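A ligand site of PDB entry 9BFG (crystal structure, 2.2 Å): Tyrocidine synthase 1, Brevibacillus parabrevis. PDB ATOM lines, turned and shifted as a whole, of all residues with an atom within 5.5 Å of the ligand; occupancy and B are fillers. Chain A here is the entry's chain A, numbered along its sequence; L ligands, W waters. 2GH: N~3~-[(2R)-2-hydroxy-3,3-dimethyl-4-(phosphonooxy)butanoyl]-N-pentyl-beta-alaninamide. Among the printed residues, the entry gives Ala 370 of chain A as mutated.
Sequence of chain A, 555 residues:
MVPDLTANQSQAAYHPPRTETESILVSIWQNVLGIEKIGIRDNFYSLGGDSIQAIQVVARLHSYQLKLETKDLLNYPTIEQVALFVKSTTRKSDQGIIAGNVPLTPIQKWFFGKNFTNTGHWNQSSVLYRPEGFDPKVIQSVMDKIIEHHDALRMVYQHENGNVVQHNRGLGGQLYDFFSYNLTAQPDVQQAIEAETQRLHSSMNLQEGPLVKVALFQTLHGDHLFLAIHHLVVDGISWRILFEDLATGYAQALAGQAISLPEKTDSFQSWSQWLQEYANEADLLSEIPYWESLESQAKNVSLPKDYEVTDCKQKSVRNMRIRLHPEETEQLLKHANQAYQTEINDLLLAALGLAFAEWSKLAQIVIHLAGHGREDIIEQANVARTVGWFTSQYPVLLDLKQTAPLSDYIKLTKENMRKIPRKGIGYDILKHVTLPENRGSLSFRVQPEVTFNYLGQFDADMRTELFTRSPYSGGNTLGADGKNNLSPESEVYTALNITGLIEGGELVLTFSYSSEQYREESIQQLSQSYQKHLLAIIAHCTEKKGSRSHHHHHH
Water W3 lies within hydrogen-bond range of O of Ala 370 (2.6 Å), N of Tyr 454 (2.9 Å) and OAG of the ligand (3.1 Å).
Water W2 lies within hydrogen-bond range of OE2 of Glu 375 (2.6 Å), NE2 of His 372 (2.7 Å) and OAH of the ligand (3.2 Å).
Water W4 bridges an oxygen (OAD) of the ligand (3.2 Å) and the backbone NH of Gly 236 (3.3 Å).
Water W1 bridges the backbone carbonyl oxygen (O) of Leu 455 and an oxygen (OAD) of the ligand.
ND2 of Asn 345 is in hydrogen-bond range of OAG of the ligand.
The backbone carbonyl oxygen (O) of Tyr 454 sits at hydrogen-bond distance from a nitrogen (NAR) of the ligand (2.6 Å).
The side-chain amide oxygen of Asn 453 lies within hydrogen-bond range of a nitrogen (NAQ) of the ligand.
NE2 of His 231 is bonded to CAA of the ligand.
OAI of the ligand is in hydrogen-bond range of N of Ser 51, 3.1 Å away.
OG of Ser 51 is covalently linked to PAX of the ligand (1.5 Å).
OAE of the ligand is in hydrogen-bond range of N of His 372 (2.9 Å).
Asp 50 touches the ligand (CB to OAI, 3.9 Å).
Ile 52 touches the ligand (CD1 to CAB, 3.7 Å).
Gln 124 touches the ligand (CD to CAA, 3.1 Å).
Ile 344 touches the ligand.
CB of Ala 370 touches NAQ of the ligand (3.8 Å).
Gly 371 touches the ligand (CA to OAE, 3.5 Å).
Thr 391 touches the ligand.
Lys 423 touches the ligand (CE to OAH, 3.6 Å).
CG of Leu 455 touches CAM of the ligand (3.9 Å).
Gly 456 touches the ligand.
Hydrophobic or aromatic side chains that line the ligand: Ile 52, His 231, Ile 344, Ala 370, His 372, Tyr 454 and Leu 455.
16 residues have an atom within 4 Å of the ligand: Asp 50, Ser 51, Ile 52, Gln 124, His 231, Ile 344, Asn 345, Ala 370, Gly 371, His 372, Thr 391, Lys 423, Asn 453, Tyr 454, Leu 455 and Gly 456.
The nearest printed residue that does not touch the ligand is Leu 478 (4.2 Å).
The backbone carbonyl oxygen of Leu 478 is in hydrogen-bond range of the side-chain amide nitrogen of Gln 124, at 2.7 Å.
The backbone carbonyl oxygen (O) of Val 234 sits at hydrogen-bond distance from a ring nitrogen (ND1) of His 231 (2.9 Å).
NE1 of Trp 389 sits close to ND1 of His 231 (3.4 Å).
NZ of Lys 423 is in salt-bridge range of OE1 of Glu 343 (2.9 Å).
OG of Ser 51 is in hydrogen-bond range of NE2 of His 372, 3.4 Å away.
N of Ile 52 is in hydrogen-bond range of OD1 of Asp 50, 2.9 Å away.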
ATOM      1  N   ASP A  50     -13.209 -16.334 -18.225  1.00  0.00           N
ATOM      2  CA  ASP A  50     -12.922 -15.447 -17.073  1.00  0.00           C
ATOM      3  C   ASP A  50     -11.410 -15.283 -16.983  1.00  0.00           C
ATOM      4  O   ASP A  50     -10.684 -15.789 -17.859  1.00  0.00           O
ATOM      5  CB  ASP A  50     -13.614 -15.951 -15.814  1.00  0.00           C
ATOM      6  CG  ASP A  50     -13.126 -17.315 -15.331  1.00  0.00           C
ATOM      7  OD1 ASP A  50     -11.946 -17.661 -15.642  1.00  0.00           O
ATOM      8  OD2 ASP A  50     -13.943 -18.048 -14.701  1.00  0.00           O
ATOM      9  N   SER A  51     -10.921 -14.564 -15.973  1.00  0.00           N
ATOM     10  CA  SER A  51      -9.476 -14.277 -15.856  1.00  0.00           C
ATOM     11  C   SER A  51      -8.678 -15.577 -15.637  1.00  0.00           C
ATOM     12  O   SER A  51      -7.512 -15.624 -16.010  1.00  0.00           O
ATOM     13  CB  SER A  51      -9.206 -13.249 -14.794  1.00  0.00           C
ATOM     14  OG  SER A  51      -9.797 -13.629 -13.575  1.00  0.00           O
ATOM     15  N   ILE A  52      -9.285 -16.619 -15.064  1.00  0.00           N
ATOM     16  CA  ILE A  52      -8.566 -17.906 -14.862  1.00  0.00           C
ATOM     17  C   ILE A  52      -8.354 -18.531 -16.234  1.00  0.00           C
ATOM     18  O   ILE A  52      -7.254 -19.007 -16.514  1.00  0.00           O
ATOM     19  CB  ILE A  52      -9.319 -18.805 -13.867  1.00  0.00           C
ATOM     20  CG1 ILE A  52      -9.162 -18.237 -12.448  1.00  0.00           C
ATOM     21  CG2 ILE A  52      -8.808 -20.237 -13.958  1.00  0.00           C
ATOM     22  CD1 ILE A  52      -9.988 -18.949 -11.432  1.00  0.00           C
ATOM     23  N   GLN A 124      -6.186 -29.266   0.123  1.00  0.00           N
ATOM     24  CA  GLN A 124      -7.169 -29.369  -0.958  1.00  0.00           C
ATOM     25  C   GLN A 124      -7.107 -30.790  -1.492  1.00  0.00           C
ATOM     26  O   GLN A 124      -6.062 -31.437  -1.368  1.00  0.00           O
ATOM     27  CB  GLN A 124      -6.869 -28.400  -2.106  1.00  0.00           C
ATOM     28  CG  GLN A 124      -7.174 -26.954  -1.790  1.00  0.00           C
ATOM     29  CD  GLN A 124      -6.950 -26.074  -3.004  1.00  0.00           C
ATOM     30  OE1 GLN A 124      -5.848 -25.867  -3.463  1.00  0.00           O
ATOM     31  NE2 GLN A 124      -8.025 -25.635  -3.603  1.00  0.00           N
ATOM     32  N   HIS A 231      -2.520 -27.179   1.438  1.00  0.00           N
ATOM     33  CA  HIS A 231      -2.800 -25.875   0.784  1.00  0.00           C
ATOM     34  C   HIS A 231      -1.523 -25.038   0.623  1.00  0.00           C
ATOM     35  O   HIS A 231      -1.516 -24.158  -0.263  1.00  0.00           O
ATOM     36  CB  HIS A 231      -3.879 -25.080   1.494  1.00  0.00           C
ATOM     37  CG  HIS A 231      -4.660 -24.297   0.509  1.00  0.00           C
ATOM     38  ND1 HIS A 231      -4.087 -23.832  -0.654  1.00  0.00           N
ATOM     39  CD2 HIS A 231      -5.966 -23.974   0.445  1.00  0.00           C
ATOM     40  CE1 HIS A 231      -4.995 -23.163  -1.337  1.00  0.00           C
ATOM     41  NE2 HIS A 231      -6.164 -23.355  -0.762  1.00  0.00           N
ATOM     42  N   VAL A 234      -0.261 -25.267  -3.137  1.00  0.00           N
ATOM     43  CA  VAL A 234      -1.218 -25.474  -4.261  1.00  0.00           C
ATOM     44  C   VAL A 234      -2.366 -24.475  -4.145  1.00  0.00           C
ATOM     45  O   VAL A 234      -2.526 -23.828  -3.058  1.00  0.00           O
ATOM     46  CB  VAL A 234      -1.679 -26.947  -4.260  1.00  0.00           C
ATOM     47  CG1 VAL A 234      -2.683 -27.245  -3.151  1.00  0.00           C
ATOM     48  CG2 VAL A 234      -2.176 -27.416  -5.624  1.00  0.00           C
ATOM     49  N   ASP A 235      -3.108 -24.333  -5.242  1.00  0.00           N
ATOM     50  CA  ASP A 235      -4.331 -23.493  -5.326  1.00  0.00           C
ATOM     51  C   ASP A 235      -5.139 -23.979  -6.532  1.00  0.00           C
ATOM     52  O   ASP A 235      -4.705 -24.954  -7.197  1.00  0.00           O
ATOM     53  CB  ASP A 235      -3.976 -21.997  -5.359  1.00  0.00           C
ATOM     54  CG  ASP A 235      -3.261 -21.490  -6.600  1.00  0.00           C
ATOM     55  OD1 ASP A 235      -3.149 -22.266  -7.614  1.00  0.00           O
ATOM     56  OD2 ASP A 235      -2.809 -20.325  -6.541  1.00  0.00           O
ATOM     57  N   GLY A 236      -6.254 -23.327  -6.814  1.00  0.00           N
ATOM     58  CA  GLY A 236      -7.235 -23.777  -7.823  1.00  0.00           C
ATOM     59  C   GLY A 236      -6.650 -23.804  -9.227  1.00  0.00           C
ATOM     60  O   GLY A 236      -6.863 -24.811  -9.971  1.00  0.00           O
ATOM     61  N   GLU A 343     -18.218  -8.212 -15.046  1.00  0.00           N
ATOM     62  CA  GLU A 343     -17.527  -9.507 -14.905  1.00  0.00           C
ATOM     63  C   GLU A 343     -18.321 -10.305 -13.879  1.00  0.00           C
ATOM     64  O   GLU A 343     -19.067  -9.682 -13.101  1.00  0.00           O
ATOM     65  CB  GLU A 343     -16.067  -9.274 -14.516  1.00  0.00           C
ATOM     66  CG  GLU A 343     -15.366  -8.456 -15.574  1.00  0.00           C
ATOM     67  CD  GLU A 343     -13.865  -8.461 -15.515  1.00  0.00           C
ATOM     68  OE1 GLU A 343     -13.301  -7.915 -14.517  1.00  0.00           O
ATOM     69  OE2 GLU A 343     -13.265  -9.017 -16.449  1.00  0.00           O
ATOM     70  N   ILE A 344     -18.152 -11.625 -13.882  1.00  0.00           N
ATOM     71  CA  ILE A 344     -19.034 -12.547 -13.112  1.00  0.00           C
ATOM     72  C   ILE A 344     -18.992 -12.183 -11.616  1.00  0.00           C
ATOM     73  O   ILE A 344     -20.044 -12.296 -10.962  1.00  0.00           O
ATOM     74  CB  ILE A 344     -18.681 -14.020 -13.402  1.00  0.00           C
ATOM     75  CG1 ILE A 344     -19.664 -14.932 -12.667  1.00  0.00           C
ATOM     76  CG2 ILE A 344     -17.234 -14.361 -13.072  1.00  0.00           C
ATOM     77  CD1 ILE A 344     -19.864 -16.224 -13.369  1.00  0.00           C
ATOM     78  N   ASN A 345     -17.861 -11.715 -11.084  1.00  0.00           N
ATOM     79  CA  ASN A 345     -17.775 -11.305  -9.654  1.00  0.00           C
ATOM     80  C   ASN A 345     -18.759 -10.153  -9.355  1.00  0.00           C
ATOM     81  O   ASN A 345     -19.313 -10.114  -8.208  1.00  0.00           O
ATOM     82  CB  ASN A 345     -16.336 -10.971  -9.259  1.00  0.00           C
ATOM     83  CG  ASN A 345     -15.579 -12.169  -8.731  1.00  0.00           C
ATOM     84  OD1 ASN A 345     -16.142 -13.253  -8.533  1.00  0.00           O
ATOM     85  ND2 ASN A 345     -14.285 -11.994  -8.527  1.00  0.00           N
ATOM     86  N   ALA A 370     -11.776 -13.615  -2.160  1.00  0.00           N
ATOM     87  CA  ALA A 370     -10.574 -14.316  -2.655  1.00  0.00           C
ATOM     88  C   ALA A 370     -10.422 -14.007  -4.148  1.00  0.00           C
ATOM     89  O   ALA A 370     -11.445 -13.945  -4.866  1.00  0.00           O
ATOM     90  CB  ALA A 370     -10.719 -15.784  -2.387  1.00  0.00           C
ATOM     91  N   GLY A 371      -9.179 -13.814  -4.604  1.00  0.00           N
ATOM     92  CA  GLY A 371      -8.857 -13.812  -6.038  1.00  0.00           C
ATOM     93  C   GLY A 371      -7.702 -14.744  -6.358  1.00  0.00           C
ATOM     94  O   GLY A 371      -6.923 -15.044  -5.423  1.00  0.00           O
ATOM     95  N   HIS A 372      -7.550 -15.142  -7.618  1.00  0.00           N
ATOM     96  CA  HIS A 372      -6.482 -16.093  -8.018  1.00  0.00           C
ATOM     97  C   HIS A 372      -5.096 -15.545  -7.666  1.00  0.00           C
ATOM     98  O   HIS A 372      -4.181 -16.336  -7.477  1.00  0.00           O
ATOM     99  CB  HIS A 372      -6.628 -16.499  -9.487  1.00  0.00           C
ATOM    100  CG  HIS A 372      -6.502 -15.385 -10.459  1.00  0.00           C
ATOM    101  ND1 HIS A 372      -5.292 -14.808 -10.741  1.00  0.00           N
ATOM    102  CD2 HIS A 372      -7.429 -14.754 -11.224  1.00  0.00           C
ATOM    103  CE1 HIS A 372      -5.469 -13.856 -11.635  1.00  0.00           C
ATOM    104  NE2 HIS A 372      -6.763 -13.801 -11.971  1.00  0.00           N
ATOM    105  N   GLY A 373      -4.926 -14.222  -7.640  1.00  0.00           N
ATOM    106  CA  GLY A 373      -3.693 -13.561  -7.164  1.00  0.00           C
ATOM    107  C   GLY A 373      -2.521 -13.636  -8.130  1.00  0.00           C
ATOM    108  O   GLY A 373      -1.374 -13.243  -7.717  1.00  0.00           O
ATOM    109  N   GLU A 375      -1.708 -11.679 -10.641  1.00  0.00           N
ATOM    110  CA  GLU A 375      -1.850 -10.360 -11.296  1.00  0.00           C
ATOM    111  C   GLU A 375      -0.488  -9.964 -11.867  1.00  0.00           C
ATOM    112  O   GLU A 375       0.528 -10.346 -11.303  1.00  0.00           O
ATOM    113  CB  GLU A 375      -2.413  -9.367 -10.290  1.00  0.00           C
ATOM    114  CG  GLU A 375      -3.819  -9.763  -9.826  1.00  0.00           C
ATOM    115  CD  GLU A 375      -4.811  -9.798 -10.959  1.00  0.00           C
ATOM    116  OE1 GLU A 375      -4.533  -9.138 -11.932  1.00  0.00           O
ATOM    117  OE2 GLU A 375      -5.816 -10.523 -10.908  1.00  0.00           O
ATOM    118  N   TRP A 389       0.581 -21.704  -3.956  1.00  0.00           N
ATOM    119  CA  TRP A 389      -0.545 -20.997  -3.330  1.00  0.00           C
ATOM    120  C   TRP A 389      -0.421 -19.500  -3.642  1.00  0.00           C
ATOM    121  O   TRP A 389       0.259 -18.798  -2.892  1.00  0.00           O
ATOM    122  CB  TRP A 389      -0.534 -21.276  -1.823  1.00  0.00           C
ATOM    123  CG  TRP A 389      -1.804 -20.930  -1.116  1.00  0.00           C
ATOM    124  CD1 TRP A 389      -2.980 -20.555  -1.688  1.00  0.00           C
ATOM    125  CD2 TRP A 389      -2.056 -20.988   0.304  1.00  0.00           C
ATOM    126  NE1 TRP A 389      -3.947 -20.387  -0.727  1.00  0.00           N
ATOM    127  CE2 TRP A 389      -3.403 -20.642   0.501  1.00  0.00           C
ATOM    128  CE3 TRP A 389      -1.274 -21.319   1.422  1.00  0.00           C
ATOM    129  CZ2 TRP A 389      -3.982 -20.598   1.778  1.00  0.00           C
ATOM    130  CZ3 TRP A 389      -1.853 -21.314   2.675  1.00  0.00           C
ATOM    131  CH2 TRP A 389      -3.185 -20.947   2.848  1.00  0.00           C
ATOM    132  N   THR A 391      -3.142 -17.436  -4.078  1.00  0.00           N
ATOM    133  CA  THR A 391      -4.456 -16.843  -3.713  1.00  0.00           C
ATOM    134  C   THR A 391      -4.263 -15.522  -2.960  1.00  0.00           C
ATOM    135  O   THR A 391      -3.424 -15.428  -2.038  1.00  0.00           O
ATOM    136  CB  THR A 391      -5.300 -17.827  -2.896  1.00  0.00           C
ATOM    137  OG1 THR A 391      -5.411 -19.015  -3.668  1.00  0.00           O
ATOM    138  CG2 THR A 391      -6.680 -17.294  -2.630  1.00  0.00           C
ATOM    139  N   LYS A 423      -6.974  -5.912  -8.654  1.00  0.00           N
ATOM    140  CA  LYS A 423      -7.825  -7.046  -8.206  1.00  0.00           C
ATOM    141  C   LYS A 423      -7.537  -7.424  -6.739  1.00  0.00           C
ATOM    142  O   LYS A 423      -7.607  -8.597  -6.400  1.00  0.00           O
ATOM    143  CB  LYS A 423      -7.614  -8.228  -9.164  1.00  0.00           C
ATOM    144  CG  LYS A 423      -8.085  -7.999 -10.595  1.00  0.00           C
ATOM    145  CD  LYS A 423      -9.570  -8.184 -10.764  1.00  0.00           C
ATOM    146  CE  LYS A 423     -10.043  -8.074 -12.201  1.00  0.00           C
ATOM    147  NZ  LYS A 423     -11.529  -8.201 -12.299  1.00  0.00           N
ATOM    148  N   ASN A 453     -15.766 -16.809  -1.938  1.00  0.00           N
ATOM    149  CA  ASN A 453     -14.681 -17.503  -2.661  1.00  0.00           C
ATOM    150  C   ASN A 453     -15.301 -18.237  -3.845  1.00  0.00           C
ATOM    151  O   ASN A 453     -15.737 -19.388  -3.648  1.00  0.00           O
ATOM    152  CB  ASN A 453     -13.899 -18.341  -1.650  1.00  0.00           C
ATOM    153  CG  ASN A 453     -12.560 -18.830  -2.136  1.00  0.00           C
ATOM    154  OD1 ASN A 453     -12.235 -18.787  -3.334  1.00  0.00           O
ATOM    155  ND2 ASN A 453     -11.774 -19.287  -1.193  1.00  0.00           N
ATOM    156  N   TYR A 454     -15.297 -17.622  -5.032  1.00  0.00           N
ATOM    157  CA  TYR A 454     -15.711 -18.269  -6.301  1.00  0.00           C
ATOM    158  C   TYR A 454     -14.468 -18.821  -6.994  1.00  0.00           C
ATOM    159  O   TYR A 454     -13.634 -18.055  -7.556  1.00  0.00           O
ATOM    160  CB  TYR A 454     -16.510 -17.315  -7.200  1.00  0.00           C
ATOM    161  CG  TYR A 454     -16.836 -17.889  -8.565  1.00  0.00           C
ATOM    162  CD1 TYR A 454     -17.435 -19.134  -8.714  1.00  0.00           C
ATOM    163  CD2 TYR A 454     -16.490 -17.203  -9.714  1.00  0.00           C
ATOM    164  CE1 TYR A 454     -17.684 -19.688  -9.968  1.00  0.00           C
ATOM    165  CE2 TYR A 454     -16.751 -17.736 -10.974  1.00  0.00           C
ATOM    166  CZ  TYR A 454     -17.340 -18.975 -11.104  1.00  0.00           C
ATOM    167  OH  TYR A 454     -17.552 -19.467 -12.354  1.00  0.00           O
ATOM    168  N   LEU A 455     -14.332 -20.144  -6.954  1.00  0.00           N
ATOM    169  CA  LEU A 455     -13.099 -20.835  -7.441  1.00  0.00           C
ATOM    170  C   LEU A 455     -13.068 -20.856  -8.972  1.00  0.00           C
ATOM    171  O   LEU A 455     -11.994 -21.047  -9.541  1.00  0.00           O
ATOM    172  CB  LEU A 455     -13.064 -22.259  -6.873  1.00  0.00           C
ATOM    173  CG  LEU A 455     -12.445 -22.377  -5.475  1.00  0.00           C
ATOM    174  CD1 LEU A 455     -13.432 -21.902  -4.405  1.00  0.00           C
ATOM    175  CD2 LEU A 455     -11.991 -23.806  -5.214  1.00  0.00           C
ATOM    176  N   GLY A 456     -14.217 -20.665  -9.605  1.00  0.00           N
ATOM    177  CA  GLY A 456     -14.304 -20.651 -11.073  1.00  0.00           C
ATOM    178  C   GLY A 456     -14.748 -21.984 -11.632  1.00  0.00           C
ATOM    179  O   GLY A 456     -15.460 -22.716 -10.940  1.00  0.00           O
ATOM    180  N   LEU A 478     -11.890 -29.083  -3.702  1.00  0.00           N
ATOM    181  CA  LEU A 478     -10.963 -27.950  -3.918  1.00  0.00           C
ATOM    182  C   LEU A 478     -11.418 -26.746  -3.095  1.00  0.00           C
ATOM    183  O   LEU A 478     -10.565 -25.960  -2.748  1.00  0.00           O
ATOM    184  CB  LEU A 478     -10.954 -27.635  -5.410  1.00  0.00           C
ATOM    185  CG  LEU A 478     -10.474 -28.778  -6.294  1.00  0.00           C
ATOM    186  CD1 LEU A 478     -10.449 -28.361  -7.763  1.00  0.00           C
ATOM    187  CD2 LEU A 478      -9.104 -29.268  -5.867  1.00  0.00           C
HETATM  188  OAH 2GH L   1     -10.295 -11.612 -12.458  1.00  0.00           O
HETATM  189  PAX 2GH L   1     -10.919 -12.948 -12.934  1.00  0.00           P
HETATM  190  OAI 2GH L   1     -12.209 -12.921 -13.711  1.00  0.00           O
HETATM  191  OAS 2GH L   1     -11.179 -13.792 -11.599  1.00  0.00           O
HETATM  192  CAP 2GH L   1     -11.552 -15.187 -11.711  1.00  0.00           C
HETATM  193  CAW 2GH L   1     -12.735 -15.422 -10.781  1.00  0.00           C
HETATM  194  CAB 2GH L   1     -13.018 -16.932 -10.737  1.00  0.00           C
HETATM  195  CAC 2GH L   1     -13.945 -14.681 -11.352  1.00  0.00           C
HETATM  196  CAV 2GH L   1     -12.451 -14.861  -9.375  1.00  0.00           C
HETATM  197  OAG 2GH L   1     -13.581 -14.989  -8.519  1.00  0.00           O
HETATM  198  CAU 2GH L   1     -11.252 -15.525  -8.739  1.00  0.00           C
HETATM  199  OAE 2GH L   1     -10.100 -15.163  -9.016  1.00  0.00           O
HETATM  200  NAR 2GH L   1     -11.534 -16.532  -7.933  1.00  0.00           N
HETATM  201  CAN 2GH L   1     -10.522 -17.484  -7.506  1.00  0.00           C
HETATM  202  CAO 2GH L   1     -10.225 -17.382  -6.037  1.00  0.00           C
HETATM  203  CAT 2GH L   1      -9.481 -18.604  -5.552  1.00  0.00           C
HETATM  204  OAD 2GH L   1      -8.765 -19.237  -6.339  1.00  0.00           O
HETATM  205  NAQ 2GH L   1      -9.670 -18.915  -4.257  1.00  0.00           N
HETATM  206  CAM 2GH L   1      -9.746 -20.254  -3.696  1.00  0.00           C
HETATM  207  CAL 2GH L   1      -8.435 -21.016  -3.725  1.00  0.00           C
HETATM  208  CAK 2GH L   1      -8.607 -22.305  -3.018  1.00  0.00           C
HETATM  209  CAJ 2GH L   1      -8.160 -22.187  -1.581  1.00  0.00           C
HETATM  210  CAA 2GH L   1      -7.408 -23.439  -1.478  1.00  0.00           C
HETATM  211  O   HOH W   1      -9.424 -21.346  -8.774  1.00  0.00           O
HETATM  212  O   HOH W   2      -7.158 -11.320 -13.040  1.00  0.00           O
HETATM  213  O   HOH W   3     -13.655 -15.235  -5.463  1.00  0.00           O
HETATM  214  O   HOH W   4      -6.333 -20.345  -8.116  1.00  0.00           O
HETATM  215  O   HOH W   5      -9.306 -12.579  -9.271  1.00  0.00           O
